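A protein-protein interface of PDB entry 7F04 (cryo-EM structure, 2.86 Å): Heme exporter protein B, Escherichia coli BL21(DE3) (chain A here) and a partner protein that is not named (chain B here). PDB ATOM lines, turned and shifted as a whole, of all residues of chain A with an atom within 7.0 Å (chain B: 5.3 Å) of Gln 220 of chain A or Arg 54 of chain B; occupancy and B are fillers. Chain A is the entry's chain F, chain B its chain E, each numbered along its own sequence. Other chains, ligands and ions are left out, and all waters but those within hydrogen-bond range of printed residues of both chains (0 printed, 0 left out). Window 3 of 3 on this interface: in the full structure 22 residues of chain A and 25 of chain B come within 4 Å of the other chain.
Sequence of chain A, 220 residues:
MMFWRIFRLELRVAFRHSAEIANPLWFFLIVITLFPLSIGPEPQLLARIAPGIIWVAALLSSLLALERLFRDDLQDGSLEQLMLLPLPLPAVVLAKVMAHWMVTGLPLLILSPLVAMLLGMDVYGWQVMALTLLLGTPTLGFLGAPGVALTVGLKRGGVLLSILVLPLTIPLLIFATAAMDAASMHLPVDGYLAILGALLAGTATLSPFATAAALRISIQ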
ATOM      1  N   LEU A  74      26.984  18.754 -20.368  1.00  0.00           N
ATOM      2  CA  LEU A  74      26.030  17.987 -21.154  1.00  0.00           C
ATOM      3  C   LEU A  74      26.132  18.317 -22.637  1.00  0.00           C
ATOM      4  O   LEU A  74      25.942  17.433 -23.479  1.00  0.00           O
ATOM      5  CB  LEU A  74      24.611  18.236 -20.648  1.00  0.00           C
ATOM      6  CG  LEU A  74      23.532  17.398 -21.330  1.00  0.00           C
ATOM      7  CD1 LEU A  74      23.750  15.918 -21.052  1.00  0.00           C
ATOM      8  CD2 LEU A  74      22.157  17.836 -20.886  1.00  0.00           C
ATOM      9  N   LEU A  82      31.164   9.409 -17.099  1.00  0.00           N
ATOM     10  CA  LEU A  82      30.319   8.249 -16.851  1.00  0.00           C
ATOM     11  C   LEU A  82      30.810   7.047 -17.644  1.00  0.00           C
ATOM     12  O   LEU A  82      30.991   5.955 -17.094  1.00  0.00           O
ATOM     13  CB  LEU A  82      28.871   8.566 -17.230  1.00  0.00           C
ATOM     14  CG  LEU A  82      28.011   9.497 -16.375  1.00  0.00           C
ATOM     15  CD1 LEU A  82      28.258  10.946 -16.731  1.00  0.00           C
ATOM     16  CD2 LEU A  82      26.548   9.160 -16.564  1.00  0.00           C
ATOM     17  N   LEU A 215      22.681  12.132 -12.471  1.00  0.00           N
ATOM     18  CA  LEU A 215      23.408  12.296 -13.724  1.00  0.00           C
ATOM     19  C   LEU A 215      23.154  11.127 -14.664  1.00  0.00           C
ATOM     20  O   LEU A 215      23.016  11.319 -15.877  1.00  0.00           O
ATOM     21  CB  LEU A 215      24.903  12.448 -13.446  1.00  0.00           C
ATOM     22  CG  LEU A 215      25.357  13.795 -12.884  1.00  0.00           C
ATOM     23  CD1 LEU A 215      26.844  13.771 -12.589  1.00  0.00           C
ATOM     24  CD2 LEU A 215      25.019  14.921 -13.842  1.00  0.00           C
ATOM     25  N   ARG A 216      23.097   9.907 -14.125  1.00  0.00           N
ATOM     26  CA  ARG A 216      22.757   8.757 -14.956  1.00  0.00           C
ATOM     27  C   ARG A 216      21.347   8.884 -15.516  1.00  0.00           C
ATOM     28  O   ARG A 216      21.093   8.516 -16.668  1.00  0.00           O
ATOM     29  CB  ARG A 216      22.903   7.464 -14.157  1.00  0.00           C
ATOM     30  CG  ARG A 216      24.328   7.163 -13.738  1.00  0.00           C
ATOM     31  CD  ARG A 216      24.648   5.686 -13.852  1.00  0.00           C
ATOM     32  NE  ARG A 216      26.083   5.453 -13.948  1.00  0.00           N
ATOM     33  CZ  ARG A 216      26.772   5.470 -15.082  1.00  0.00           C
ATOM     34  NH1 ARG A 216      26.181   5.685 -16.245  1.00  0.00           N
ATOM     35  NH2 ARG A 216      28.085   5.265 -15.045  1.00  0.00           N
ATOM     36  N   ILE A 217      20.414   9.398 -14.712  1.00  0.00           N
ATOM     37  CA  ILE A 217      19.057   9.629 -15.205  1.00  0.00           C
ATOM     38  C   ILE A 217      19.071  10.646 -16.339  1.00  0.00           C
ATOM     39  O   ILE A 217      18.423  10.455 -17.375  1.00  0.00           O
ATOM     40  CB  ILE A 217      18.132  10.086 -14.060  1.00  0.00           C
ATOM     41  CG1 ILE A 217      18.059   9.043 -12.942  1.00  0.00           C
ATOM     42  CG2 ILE A 217      16.746  10.402 -14.589  1.00  0.00           C
ATOM     43  CD1 ILE A 217      18.004   7.614 -13.413  1.00  0.00           C
ATOM     44  N   SER A 218      19.814  11.740 -16.164  1.00  0.00           N
ATOM     45  CA  SER A 218      19.759  12.843 -17.117  1.00  0.00           C
ATOM     46  C   SER A 218      20.494  12.527 -18.413  1.00  0.00           C
ATOM     47  O   SER A 218      20.116  13.038 -19.473  1.00  0.00           O
ATOM     48  CB  SER A 218      20.336  14.110 -16.486  1.00  0.00           C
ATOM     49  OG  SER A 218      19.684  14.412 -15.266  1.00  0.00           O
ATOM     50  N   ILE A 219      21.546  11.707 -18.356  1.00  0.00           N
ATOM     51  CA  ILE A 219      22.325  11.434 -19.561  1.00  0.00           C
ATOM     52  C   ILE A 219      21.503  10.651 -20.577  1.00  0.00           C
ATOM     53  O   ILE A 219      21.760  10.729 -21.785  1.00  0.00           O
ATOM     54  CB  ILE A 219      23.634  10.705 -19.199  1.00  0.00           C
ATOM     55  CG1 ILE A 219      24.661  10.866 -20.319  1.00  0.00           C
ATOM     56  CG2 ILE A 219      23.383   9.230 -18.933  1.00  0.00           C
ATOM     57  CD1 ILE A 219      25.162  12.281 -20.484  1.00  0.00           C
ATOM     58  N   GLN A 220      20.505   9.898 -20.123  1.00  0.00           N
ATOM     59  CA  GLN A 220      19.664   9.117 -21.022  1.00  0.00           C
ATOM     60  C   GLN A 220      18.406   9.889 -21.403  1.00  0.00           C
ATOM     61  O   GLN A 220      18.315  10.444 -22.499  1.00  0.00           O
ATOM     62  CB  GLN A 220      19.287   7.782 -20.379  1.00  0.00           C
ATOM     63  CG  GLN A 220      20.413   7.133 -19.598  1.00  0.00           C
ATOM     64  CD  GLN A 220      19.927   6.026 -18.685  1.00  0.00           C
ATOM     65  OE1 GLN A 220      18.742   5.697 -18.668  1.00  0.00           O
ATOM     66  NE2 GLN A 220      20.843   5.448 -17.918  1.00  0.00           N
ATOM     67  N   ARG B  47      25.363   4.064 -27.785  1.00  0.00           N
ATOM     68  CA  ARG B  47      25.306   4.435 -26.377  1.00  0.00           C
ATOM     69  C   ARG B  47      24.939   3.246 -25.499  1.00  0.00           C
ATOM     70  O   ARG B  47      25.264   3.232 -24.308  1.00  0.00           O
ATOM     71  CB  ARG B  47      24.312   5.575 -26.180  1.00  0.00           C
ATOM     72  CG  ARG B  47      24.692   6.842 -26.915  1.00  0.00           C
ATOM     73  CD  ARG B  47      23.826   7.999 -26.483  1.00  0.00           C
ATOM     74  NE  ARG B  47      23.539   7.946 -25.057  1.00  0.00           N
ATOM     75  CZ  ARG B  47      23.670   8.974 -24.231  1.00  0.00           C
ATOM     76  NH1 ARG B  47      24.113  10.146 -24.652  1.00  0.00           N
ATOM     77  NH2 ARG B  47      23.351   8.821 -22.949  1.00  0.00           N
ATOM     78  N   LEU B  48      24.260   2.249 -26.065  1.00  0.00           N
ATOM     79  CA  LEU B  48      24.007   1.013 -25.331  1.00  0.00           C
ATOM     80  C   LEU B  48      25.280   0.194 -25.190  1.00  0.00           C
ATOM     81  O   LEU B  48      25.511  -0.435 -24.152  1.00  0.00           O
ATOM     82  CB  LEU B  48      22.924   0.200 -26.038  1.00  0.00           C
ATOM     83  CG  LEU B  48      21.505   0.256 -25.476  1.00  0.00           C
ATOM     84  CD1 LEU B  48      21.024   1.691 -25.352  1.00  0.00           C
ATOM     85  CD2 LEU B  48      20.570  -0.540 -26.362  1.00  0.00           C
ATOM     86  N   GLY B  51      27.484   1.533 -22.485  1.00  0.00           N
ATOM     87  CA  GLY B  51      26.896   1.493 -21.167  1.00  0.00           C
ATOM     88  C   GLY B  51      26.296   2.794 -20.689  1.00  0.00           C
ATOM     89  O   GLY B  51      25.807   2.847 -19.554  1.00  0.00           O
ATOM     90  N   LEU B  52      26.322   3.846 -21.508  1.00  0.00           N
ATOM     91  CA  LEU B  52      25.733   5.117 -21.099  1.00  0.00           C
ATOM     92  C   LEU B  52      24.230   4.990 -20.894  1.00  0.00           C
ATOM     93  O   LEU B  52      23.676   5.549 -19.941  1.00  0.00           O
ATOM     94  CB  LEU B  52      26.041   6.197 -22.132  1.00  0.00           C
ATOM     95  CG  LEU B  52      27.474   6.723 -22.145  1.00  0.00           C
ATOM     96  CD1 LEU B  52      27.816   7.299 -23.504  1.00  0.00           C
ATOM     97  CD2 LEU B  52      27.656   7.761 -21.054  1.00  0.00           C
ATOM     98  N   SER B  53      23.555   4.262 -21.778  1.00  0.00           N
ATOM     99  CA  SER B  53      22.122   4.034 -21.685  1.00  0.00           C
ATOM    100  C   SER B  53      21.855   2.551 -21.487  1.00  0.00           C
ATOM    101  O   SER B  53      22.465   1.707 -22.150  1.00  0.00           O
ATOM    102  CB  SER B  53      21.401   4.534 -22.937  1.00  0.00           C
ATOM    103  OG  SER B  53      21.451   5.947 -23.026  1.00  0.00           O
ATOM    104  N   ARG B  54      20.950   2.237 -20.565  1.00  0.00           N
ATOM    105  CA  ARG B  54      20.667   0.814 -20.435  1.00  0.00           C
ATOM    106  C   ARG B  54      19.537   0.409 -21.379  1.00  0.00           C
ATOM    107  O   ARG B  54      18.604   1.185 -21.601  1.00  0.00           O
ATOM    108  CB  ARG B  54      20.293   0.464 -18.996  1.00  0.00           C
ATOM    109  CG  ARG B  54      19.078   1.190 -18.450  1.00  0.00           C
ATOM    110  CD  ARG B  54      18.815   0.781 -17.010  1.00  0.00           C
ATOM    111  NE  ARG B  54      17.593   1.371 -16.481  1.00  0.00           N
ATOM    112  CZ  ARG B  54      17.540   2.519 -15.819  1.00  0.00           C
ATOM    113  NH1 ARG B  54      18.630   3.226 -15.573  1.00  0.00           N
ATOM    114  NH2 ARG B  54      16.362   2.966 -15.390  1.00  0.00           N
ATOM    115  N   PRO B  55      19.609  -0.789 -21.952  1.00  0.00           N
ATOM    116  CA  PRO B  55      18.598  -1.203 -22.929  1.00  0.00           C
ATOM    117  C   PRO B  55      17.243  -1.433 -22.280  1.00  0.00           C
ATOM    118  O   PRO B  55      17.129  -1.708 -21.084  1.00  0.00           O
ATOM    119  CB  PRO B  55      19.160  -2.511 -23.500  1.00  0.00           C
ATOM    120  CG  PRO B  55      20.582  -2.581 -23.034  1.00  0.00           C
ATOM    121  CD  PRO B  55      20.635  -1.822 -21.755  1.00  0.00           C
ATOM    122  N   ASP B  56      16.199  -1.302 -23.101  1.00  0.00           N
ATOM    123  CA  ASP B  56      14.865  -1.693 -22.659  1.00  0.00           C
ATOM    124  C   ASP B  56      14.805  -3.187 -22.377  1.00  0.00           C
ATOM    125  O   ASP B  56      14.184  -3.622 -21.401  1.00  0.00           O
ATOM    126  CB  ASP B  56      13.826  -1.300 -23.708  1.00  0.00           C
ATOM    127  CG  ASP B  56      13.699   0.204 -23.869  1.00  0.00           C
ATOM    128  OD1 ASP B  56      14.573   0.934 -23.359  1.00  0.00           O
ATOM    129  OD2 ASP B  56      12.724   0.656 -24.504  1.00  0.00           O
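Along chain B the printed residues that touch a printed residue of chain A span positions 47 to 54.
Of the 8 printed residues of chain A, 2 touch a printed residue of chain B.
Hydrophobic or aromatic side chains of chain A within 4 Å of the printed part of chain B: Ile 219.
Arg 216 of chain A touches none of the printed residues of chain B.
Printed residues of chain B within 4 Å of Ile 219 of chain A: Arg 47 (2.7 Å) and Leu 52 (3.8 Å).
Of chain B, only Leu 52, Ser 53 and Arg 54 come within 4 Å of Gln 220 of chain A.
Of the printed residues of chain A, Arg 47 of chain B touches Ile 219.
Of chain A, only Gln 220 comes within 4 Å of Arg 54 of chain B.
Asp 56 of chain B touches none of the printed residues of chain A.
The nearest residue of chain B that does not touch Gln 220 of chain A is Arg 47 of chain B (4.2 Å).
The side-chain amide nitrogen (NE2) of Gln 220 of chain A lies close to the backbone carbonyl oxygen (O) of Arg 216 of chain A (3.3 Å).
O of Arg 47 of chain B sits at hydrogen-bond distance from N of Ser 53 of chain B, at 3.2 Å.
The backbone carbonyl oxygen (O) of Arg 47 of chain B sits at hydrogen-bond distance from the backbone NH (N) of Leu 52 of chain B, 3.1 Å away.
The guanidinium group (NH2) of Arg 47 of chain B is in hydrogen-bond range of the backbone carbonyl oxygen (O) of Ile 219 of chain A, at 2.7 Å.
The side-chain amide nitrogen (NE2) of Gln 220 of chain A is in hydrogen-bond range of the backbone carbonyl oxygen (O) of Leu 52 of chain B (3.5 Å).
Ile 219 of chain A touches Leu 52 of chain B.
CG of Gln 220 of chain A touches OG of Ser 53 of chain B (3.8 Å).
Arg 54 of chain B touches Gln 220 of chain A.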
